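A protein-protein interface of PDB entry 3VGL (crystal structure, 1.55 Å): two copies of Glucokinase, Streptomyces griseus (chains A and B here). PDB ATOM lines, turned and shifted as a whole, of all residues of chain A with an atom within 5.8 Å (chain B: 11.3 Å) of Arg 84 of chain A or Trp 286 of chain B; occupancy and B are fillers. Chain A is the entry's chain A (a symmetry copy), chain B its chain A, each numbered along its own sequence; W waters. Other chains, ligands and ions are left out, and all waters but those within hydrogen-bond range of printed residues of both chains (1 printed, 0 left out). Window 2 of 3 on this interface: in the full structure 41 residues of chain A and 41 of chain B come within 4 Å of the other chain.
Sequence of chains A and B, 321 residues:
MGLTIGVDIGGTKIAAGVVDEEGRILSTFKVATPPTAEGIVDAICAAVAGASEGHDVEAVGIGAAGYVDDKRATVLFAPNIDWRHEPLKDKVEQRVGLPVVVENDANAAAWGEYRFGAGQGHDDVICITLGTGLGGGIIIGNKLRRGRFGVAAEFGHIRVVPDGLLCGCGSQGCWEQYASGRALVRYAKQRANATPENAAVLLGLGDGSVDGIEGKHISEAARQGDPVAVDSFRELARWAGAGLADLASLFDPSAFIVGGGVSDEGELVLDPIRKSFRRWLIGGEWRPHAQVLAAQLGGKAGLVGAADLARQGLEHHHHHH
Along chain A the printed residues that touch a printed residue of chain B span positions 76 to 85.
Of the 12 printed residues of chain B, 2 touch a printed residue of chain A.
Hydrophobic or aromatic side chains of chain B that line the printed part of chain A: Trp 286.
Among the printed residues, 5 pairs touch across the chains.
Among the printed residues, no Asp or Glu carboxylate lies within 4 Å of a Lys or Arg side-chain nitrogen of the other chain.
Arg 84 of chain A touches just one residue of chain B: Trp 286.
Trp 286 of chain B touches just these residues of chain A: Leu 76 (3.8 Å), Phe 77 (3.7 Å), Arg 84 (3.6 Å) and His 85 (2.9 Å).
Phe 77 of chain A touches just these residues of chain B: Gly 283 and Trp 286.
No residue of chain B comes within 4 Å of Asp 82 of chain A.
Of chain B, only Trp 286 (2.9 Å) comes within 4 Å of His 85 of chain A.
No residue of chain B comes within 4 Å of Glu 86 of chain A.
Of the printed residues of chain A, Gly 283 of chain B touches Phe 77 (3.8 Å).
Arg 278 of chain B touches none of the printed residues of chain A.
The nearest residue of chain B that does not touch Arg 84 of chain A is Gly 283 of chain B (6.5 Å).
No position is printed for both chains.
The backbone carbonyl oxygen (O) of Val 75 of chain A sits at hydrogen-bond distance from the backbone NH (N) of His 85 of chain A (3.1 Å).
The backbone carbonyl oxygen (O) of Leu 76 of chain A sits at hydrogen-bond distance from the backbone NH (N) of His 85 of chain A (2.9 Å).
The backbone carbonyl oxygen of Ala 78 of chain A sits at hydrogen-bond distance from the guanidinium group of Arg 84 of chain A (2.9 Å).
Water W1 lies within hydrogen-bond range of O of Glu 285 of chain B (2.7 Å), NE2 of His 85 of chain A (3.2 Å) and O of Trp 286 of chain B (3.4 Å).
Among the printed residues, pairs that only touch across the chains: Arg 84 of chain A with Trp 286 of chain B (3.6 Å), Phe 77 of chain A with Trp 286 of chain B (3.7 Å), Leu 76 of chain A with Trp 286 of chain B (3.8 Å) and Phe 77 of chain A with Gly 283 of chain B (3.8 Å).
NE2 of His 85 of chain A sits at hydrogen-bond distance from O of Trp 286 of chain B (2.9 Å).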
ATOM      1  N   VAL A  75      -9.908   9.074 -28.149  1.00  0.00           N
ATOM      2  CA  VAL A  75      -9.980   7.736 -27.541  1.00  0.00           C
ATOM      3  C   VAL A  75     -11.425   7.505 -27.078  1.00  0.00           C
ATOM      4  O   VAL A  75     -11.847   8.061 -26.070  1.00  0.00           O
ATOM      5  CB  VAL A  75      -8.962   7.559 -26.380  1.00  0.00           C
ATOM      6  CG1 VAL A  75      -8.994   6.091 -25.877  1.00  0.00           C
ATOM      7  CG2 VAL A  75      -7.517   7.910 -26.837  1.00  0.00           C
ATOM      8  N   LEU A  76     -12.165   6.695 -27.835  1.00  0.00           N
ATOM      9  CA  LEU A  76     -13.596   6.410 -27.561  1.00  0.00           C
ATOM     10  C   LEU A  76     -13.778   5.688 -26.232  1.00  0.00           C
ATOM     11  O   LEU A  76     -14.689   5.988 -25.465  1.00  0.00           O
ATOM     12  CB  LEU A  76     -14.242   5.587 -28.695  1.00  0.00           C
ATOM     13  CG  LEU A  76     -14.268   6.215 -30.090  1.00  0.00           C
ATOM     14  CD1 LEU A  76     -14.744   5.235 -31.163  1.00  0.00           C
ATOM     15  CD2 LEU A  76     -15.155   7.463 -30.057  1.00  0.00           C
ATOM     16  N   PHE A  77     -12.896   4.733 -25.952  1.00  0.00           N
ATOM     17  CA  PHE A  77     -13.111   3.789 -24.862  1.00  0.00           C
ATOM     18  C   PHE A  77     -11.743   3.154 -24.546  1.00  0.00           C
ATOM     19  O   PHE A  77     -11.012   2.797 -25.470  1.00  0.00           O
ATOM     20  CB  PHE A  77     -14.137   2.738 -25.349  1.00  0.00           C
ATOM     21  CG  PHE A  77     -14.463   1.676 -24.359  1.00  0.00           C
ATOM     22  CD1 PHE A  77     -15.414   1.900 -23.362  1.00  0.00           C
ATOM     23  CD2 PHE A  77     -13.869   0.422 -24.453  1.00  0.00           C
ATOM     24  CE1 PHE A  77     -15.737   0.896 -22.446  1.00  0.00           C
ATOM     25  CE2 PHE A  77     -14.199  -0.602 -23.544  1.00  0.00           C
ATOM     26  CZ  PHE A  77     -15.127  -0.356 -22.537  1.00  0.00           C
ATOM     27  N   ALA A  78     -11.377   3.046 -23.266  1.00  0.00           N
ATOM     28  CA  ALA A  78     -10.172   2.243 -22.892  1.00  0.00           C
ATOM     29  C   ALA A  78     -10.439   1.345 -21.686  1.00  0.00           C
ATOM     30  O   ALA A  78     -10.999   1.803 -20.701  1.00  0.00           O
ATOM     31  CB  ALA A  78      -8.990   3.136 -22.610  1.00  0.00           C
ATOM     32  N   PRO A  79     -10.057   0.051 -21.764  1.00  0.00           N
ATOM     33  CA  PRO A  79     -10.343  -0.833 -20.634  1.00  0.00           C
ATOM     34  C   PRO A  79      -9.435  -0.659 -19.425  1.00  0.00           C
ATOM     35  O   PRO A  79      -9.856  -0.971 -18.295  1.00  0.00           O
ATOM     36  CB  PRO A  79     -10.162  -2.252 -21.223  1.00  0.00           C
ATOM     37  CG  PRO A  79      -9.375  -2.080 -22.388  1.00  0.00           C
ATOM     38  CD  PRO A  79      -9.611  -0.687 -22.950  1.00  0.00           C
ATOM     39  N   ILE A  81      -7.322   2.240 -18.862  1.00  0.00           N
ATOM     40  CA  ILE A  81      -7.004   3.656 -18.647  1.00  0.00           C
ATOM     41  C   ILE A  81      -8.362   4.370 -18.574  1.00  0.00           C
ATOM     42  O   ILE A  81      -9.291   4.001 -19.277  1.00  0.00           O
ATOM     43  CB  ILE A  81      -6.153   4.221 -19.818  1.00  0.00           C
ATOM     44  CG1 ILE A  81      -4.767   3.568 -19.854  1.00  0.00           C
ATOM     45  CG2 ILE A  81      -5.992   5.765 -19.712  1.00  0.00           C
ATOM     46  CD1 ILE A  81      -4.024   3.835 -21.117  1.00  0.00           C
ATOM     47  N   ASP A  82      -8.462   5.431 -17.783  1.00  0.00           N
ATOM     48  CA  ASP A  82      -9.750   6.131 -17.642  1.00  0.00           C
ATOM     49  C   ASP A  82     -10.001   7.151 -18.770  1.00  0.00           C
ATOM     50  O   ASP A  82      -9.923   8.383 -18.585  1.00  0.00           O
ATOM     51  CB  ASP A  82      -9.876   6.750 -16.248  1.00  0.00           C
ATOM     52  CG  ASP A  82     -11.287   7.257 -15.947  1.00  0.00           C
ATOM     53  OD1 ASP A  82     -12.284   6.737 -16.521  1.00  0.00           O
ATOM     54  OD2 ASP A  82     -11.393   8.170 -15.106  1.00  0.00           O
ATOM     55  N   TRP A  83     -10.292   6.615 -19.947  1.00  0.00           N
ATOM     56  CA  TRP A  83     -10.615   7.410 -21.126  1.00  0.00           C
ATOM     57  C   TRP A  83     -12.017   7.023 -21.605  1.00  0.00           C
ATOM     58  O   TRP A  83     -12.291   5.853 -21.873  1.00  0.00           O
ATOM     59  CB  TRP A  83      -9.614   7.120 -22.248  1.00  0.00           C
ATOM     60  CG  TRP A  83      -8.268   7.838 -22.214  1.00  0.00           C
ATOM     61  CD1 TRP A  83      -8.000   9.091 -21.736  1.00  0.00           C
ATOM     62  CD2 TRP A  83      -7.026   7.345 -22.756  1.00  0.00           C
ATOM     63  NE1 TRP A  83      -6.667   9.412 -21.941  1.00  0.00           N
ATOM     64  CE2 TRP A  83      -6.049   8.353 -22.560  1.00  0.00           C
ATOM     65  CE3 TRP A  83      -6.645   6.145 -23.370  1.00  0.00           C
ATOM     66  CZ2 TRP A  83      -4.707   8.193 -22.962  1.00  0.00           C
ATOM     67  CZ3 TRP A  83      -5.307   5.995 -23.789  1.00  0.00           C
ATOM     68  CH2 TRP A  83      -4.364   7.010 -23.575  1.00  0.00           C
ATOM     69  N   ARG A  84     -12.904   8.010 -21.729  1.00  0.00           N
ATOM     70  CA  ARG A  84     -14.198   7.792 -22.363  1.00  0.00           C
ATOM     71  C   ARG A  84     -14.451   8.999 -23.259  1.00  0.00           C
ATOM     72  O   ARG A  84     -14.631  10.104 -22.753  1.00  0.00           O
ATOM     73  CB  ARG A  84     -15.327   7.651 -21.325  1.00  0.00           C
ATOM     74  CG  ARG A  84     -15.275   6.390 -20.438  1.00  0.00           C
ATOM     75  CD  ARG A  84     -15.584   5.130 -21.228  1.00  0.00           C
ATOM     76  NE  ARG A  84     -15.594   3.930 -20.397  1.00  0.00           N
ATOM     77  CZ  ARG A  84     -14.513   3.209 -20.102  1.00  0.00           C
ATOM     78  NH1 ARG A  84     -13.307   3.577 -20.533  1.00  0.00           N
ATOM     79  NH2 ARG A  84     -14.645   2.127 -19.342  1.00  0.00           N
ATOM     80  N   HIS A  85     -14.470   8.773 -24.576  1.00  0.00           N
ATOM     81  CA  HIS A  85     -14.647   9.844 -25.572  1.00  0.00           C
ATOM     82  C   HIS A  85     -13.675  10.999 -25.285  1.00  0.00           C
ATOM     83  O   HIS A  85     -14.057  12.187 -25.249  1.00  0.00           O
ATOM     84  CB  HIS A  85     -16.119  10.319 -25.629  1.00  0.00           C
ATOM     85  CG  HIS A  85     -17.058   9.353 -26.292  1.00  0.00           C
ATOM     86  ND1 HIS A  85     -18.353   9.691 -26.607  1.00  0.00           N
ATOM     87  CD2 HIS A  85     -16.902   8.068 -26.700  1.00  0.00           C
ATOM     88  CE1 HIS A  85     -18.961   8.661 -27.168  1.00  0.00           C
ATOM     89  NE2 HIS A  85     -18.099   7.665 -27.244  1.00  0.00           N
ATOM     90  N   GLU A  86     -12.406  10.641 -25.106  1.00  0.00           N
ATOM     91  CA  GLU A  86     -11.356  11.597 -24.765  1.00  0.00           C
ATOM     92  C   GLU A  86     -10.753  12.291 -26.009  1.00  0.00           C
ATOM     93  O   GLU A  86     -10.099  11.640 -26.829  1.00  0.00           O
ATOM     94  CB  GLU A  86     -10.256  10.883 -23.957  1.00  0.00           C
ATOM     95  CG  GLU A  86      -8.998  11.725 -23.644  1.00  0.00           C
ATOM     96  CD  GLU A  86      -9.210  12.722 -22.501  1.00  0.00           C
ATOM     97  OE1 GLU A  86      -8.249  13.434 -22.139  1.00  0.00           O
ATOM     98  OE2 GLU A  86     -10.337  12.777 -21.961  1.00  0.00           O
ATOM     99  N   GLY A 168     -11.458  -5.442 -18.005  1.00  0.00           N
ATOM    100  CA  GLY A 168     -11.623  -3.998 -17.857  1.00  0.00           C
ATOM    101  C   GLY A 168     -12.616  -3.385 -18.828  1.00  0.00           C
ATOM    102  O   GLY A 168     -13.157  -2.296 -18.573  1.00  0.00           O
ATOM    103  N   ASP B 252     -14.199  -4.577 -37.394  1.00  0.00           N
ATOM    104  CA  ASP B 252     -15.000  -3.322 -37.349  1.00  0.00           C
ATOM    105  C   ASP B 252     -15.586  -2.885 -38.716  1.00  0.00           C
ATOM    106  O   ASP B 252     -15.302  -1.768 -39.188  1.00  0.00           O
ATOM    107  CB  ASP B 252     -14.155  -2.187 -36.728  1.00  0.00           C
ATOM    108  CG  ASP B 252     -14.956  -0.905 -36.483  1.00  0.00           C
ATOM    109  OD1 ASP B 252     -16.133  -1.002 -36.070  1.00  0.00           O
ATOM    110  OD2 ASP B 252     -14.383   0.198 -36.657  1.00  0.00           O
ATOM    111  N   ARG B 278     -26.059  -7.064 -30.691  1.00  0.00           N
ATOM    112  CA  ARG B 278     -26.078  -5.847 -29.889  1.00  0.00           C
ATOM    113  C   ARG B 278     -25.850  -6.096 -28.399  1.00  0.00           C
ATOM    114  O   ARG B 278     -25.227  -5.257 -27.726  1.00  0.00           O
ATOM    115  CB  ARG B 278     -27.343  -5.023 -30.129  1.00  0.00           C
ATOM    116  CG  ARG B 278     -27.430  -4.439 -31.536  1.00  0.00           C
ATOM    117  CD  ARG B 278     -26.311  -3.427 -31.858  1.00  0.00           C
ATOM    118  NE  ARG B 278     -26.240  -2.352 -30.855  1.00  0.00           N
ATOM    119  CZ  ARG B 278     -27.006  -1.268 -30.853  1.00  0.00           C
ATOM    120  NH1 ARG B 278     -27.902  -1.083 -31.804  1.00  0.00           N
ATOM    121  NH2 ARG B 278     -26.863  -0.366 -29.884  1.00  0.00           N
ATOM    122  N   LEU B 281     -21.857  -6.914 -28.159  1.00  0.00           N
ATOM    123  CA  LEU B 281     -20.882  -5.936 -28.676  1.00  0.00           C
ATOM    124  C   LEU B 281     -20.152  -5.192 -27.548  1.00  0.00           C
ATOM    125  O   LEU B 281     -20.815  -4.567 -26.732  1.00  0.00           O
ATOM    126  CB  LEU B 281     -21.623  -4.944 -29.591  1.00  0.00           C
ATOM    127  CG  LEU B 281     -20.747  -3.936 -30.332  1.00  0.00           C
ATOM    128  CD1 LEU B 281     -19.835  -4.667 -31.312  1.00  0.00           C
ATOM    129  CD2 LEU B 281     -21.653  -2.943 -31.066  1.00  0.00           C
ATOM    130  N   ILE B 282     -18.813  -5.302 -27.525  1.00  0.00           N
ATOM    131  CA  ILE B 282     -17.922  -4.741 -26.463  1.00  0.00           C
ATOM    132  C   ILE B 282     -18.108  -3.221 -26.405  1.00  0.00           C
ATOM    133  O   ILE B 282     -18.214  -2.578 -27.433  1.00  0.00           O
ATOM    134  CB  ILE B 282     -16.382  -5.009 -26.768  1.00  0.00           C
ATOM    135  CG1 ILE B 282     -16.024  -6.515 -26.814  1.00  0.00           C
ATOM    136  CG2 ILE B 282     -15.483  -4.364 -25.720  1.00  0.00           C
ATOM    137  CD1 ILE B 282     -16.261  -7.279 -25.509  1.00  0.00           C
ATOM    138  N   GLY B 283     -18.088  -2.668 -25.200  1.00  0.00           N
ATOM    139  CA  GLY B 283     -17.906  -1.231 -25.045  1.00  0.00           C
ATOM    140  C   GLY B 283     -19.209  -0.474 -24.923  1.00  0.00           C
ATOM    141  O   GLY B 283     -19.219   0.761 -24.828  1.00  0.00           O
ATOM    142  N   GLY B 284     -20.302  -1.222 -24.860  1.00  0.00           N
ATOM    143  CA  GLY B 284     -21.618  -0.668 -24.595  1.00  0.00           C
ATOM    144  C   GLY B 284     -21.937   0.539 -25.440  1.00  0.00           C
ATOM    145  O   GLY B 284     -21.925   0.456 -26.662  1.00  0.00           O
ATOM    146  N   GLU B 285     -22.172   1.667 -24.767  1.00  0.00           N
ATOM    147  CA  GLU B 285     -22.702   2.873 -25.409  1.00  0.00           C
ATOM    148  C   GLU B 285     -21.622   3.718 -26.083  1.00  0.00           C
ATOM    149  O   GLU B 285     -21.935   4.687 -26.810  1.00  0.00           O
ATOM    150  CB  GLU B 285     -23.414   3.725 -24.354  1.00  0.00           C
ATOM    151  CG  GLU B 285     -22.454   4.235 -23.260  1.00  0.00           C
ATOM    152  CD  GLU B 285     -23.132   4.837 -22.051  1.00  0.00           C
ATOM    153  OE1 GLU B 285     -23.821   5.877 -22.195  1.00  0.00           O
ATOM    154  OE2 GLU B 285     -22.937   4.286 -20.941  1.00  0.00           O
ATOM    155  N   TRP B 286     -20.364   3.331 -25.870  1.00  0.00           N
ATOM    156  CA  TRP B 286     -19.205   4.179 -26.198  1.00  0.00           C
ATOM    157  C   TRP B 286     -18.695   4.046 -27.632  1.00  0.00           C
ATOM    158  O   TRP B 286     -17.905   4.883 -28.096  1.00  0.00           O
ATOM    159  CB  TRP B 286     -18.070   3.939 -25.190  1.00  0.00           C
ATOM    160  CG  TRP B 286     -18.488   4.210 -23.794  1.00  0.00           C
ATOM    161  CD1 TRP B 286     -18.756   3.286 -22.806  1.00  0.00           C
ATOM    162  CD2 TRP B 286     -18.727   5.500 -23.210  1.00  0.00           C
ATOM    163  NE1 TRP B 286     -19.131   3.932 -21.648  1.00  0.00           N
ATOM    164  CE2 TRP B 286     -19.120   5.287 -21.865  1.00  0.00           C
ATOM    165  CE3 TRP B 286     -18.638   6.821 -23.692  1.00  0.00           C
ATOM    166  CZ2 TRP B 286     -19.424   6.344 -20.995  1.00  0.00           C
ATOM    167  CZ3 TRP B 286     -18.939   7.871 -22.831  1.00  0.00           C
ATOM    168  CH2 TRP B 286     -19.327   7.623 -21.492  1.00  0.00           C
ATOM    169  N   ARG B 287     -19.186   3.031 -28.341  1.00  0.00           N
ATOM    170  CA  ARG B 287     -18.717   2.712 -29.695  1.00  0.00           C
ATOM    171  C   ARG B 287     -19.856   2.385 -30.671  1.00  0.00           C
ATOM    172  O   ARG B 287     -20.909   1.876 -30.268  1.00  0.00           O
ATOM    173  CB  ARG B 287     -17.636   1.594 -29.669  1.00  0.00           C
ATOM    174  CG  ARG B 287     -18.029   0.256 -29.030  1.00  0.00           C
ATOM    175  CD  ARG B 287     -18.840  -0.701 -29.934  1.00  0.00           C
ATOM    176  NE  ARG B 287     -18.188  -1.091 -31.168  1.00  0.00           N
ATOM    177  CZ  ARG B 287     -17.264  -2.042 -31.287  1.00  0.00           C
ATOM    178  NH1 ARG B 287     -16.863  -2.718 -30.195  1.00  0.00           N
ATOM    179  NH2 ARG B 287     -16.730  -2.288 -32.511  1.00  0.00           N
ATOM    180  N   PRO B 288     -19.640   2.647 -31.972  1.00  0.00           N
ATOM    181  CA  PRO B 288     -20.717   2.450 -32.923  1.00  0.00           C
ATOM    182  C   PRO B 288     -20.967   0.977 -33.279  1.00  0.00           C
ATOM    183  O   PRO B 288     -20.094   0.122 -33.105  1.00  0.00           O
ATOM    184  CB  PRO B 288     -20.243   3.215 -34.173  1.00  0.00           C
ATOM    185  CG  PRO B 288     -19.047   3.998 -33.748  1.00  0.00           C
ATOM    186  CD  PRO B 288     -18.452   3.227 -32.615  1.00  0.00           C
ATOM    187  N   HIS B 289     -22.163   0.704 -33.768  1.00  0.00           N
ATOM    188  CA  HIS B 289     -22.513  -0.670 -34.146  1.00  0.00           C
ATOM    189  C   HIS B 289     -22.679  -0.830 -35.652  1.00  0.00           C
ATOM    190  O   HIS B 289     -23.287  -0.001 -36.330  1.00  0.00           O
ATOM    191  CB  HIS B 289     -23.772  -1.132 -33.423  1.00  0.00           C
ATOM    192  CG  HIS B 289     -24.942  -0.221 -33.603  1.00  0.00           C
ATOM    193  ND1 HIS B 289     -25.229   0.796 -32.719  1.00  0.00           N
ATOM    194  CD2 HIS B 289     -25.884  -0.153 -34.577  1.00  0.00           C
ATOM    195  CE1 HIS B 289     -26.302   1.447 -33.135  1.00  0.00           C
ATOM    196  NE2 HIS B 289     -26.721   0.889 -34.256  1.00  0.00           N
ATOM    197  N   ALA B 290     -22.173  -1.938 -36.174  1.00  0.00           N
ATOM    198  CA  ALA B 290     -22.396  -2.313 -37.569  1.00  0.00           C
ATOM    199  C   ALA B 290     -23.848  -2.674 -37.794  1.00  0.00           C
ATOM    200  O   ALA B 290     -24.564  -3.026 -36.851  1.00  0.00           O
ATOM    201  CB  ALA B 290     -21.536  -3.519 -37.902  1.00  0.00           C
HETATM  202  O   HOH W   1     -20.882   6.563 -28.439  1.00  0.00           O
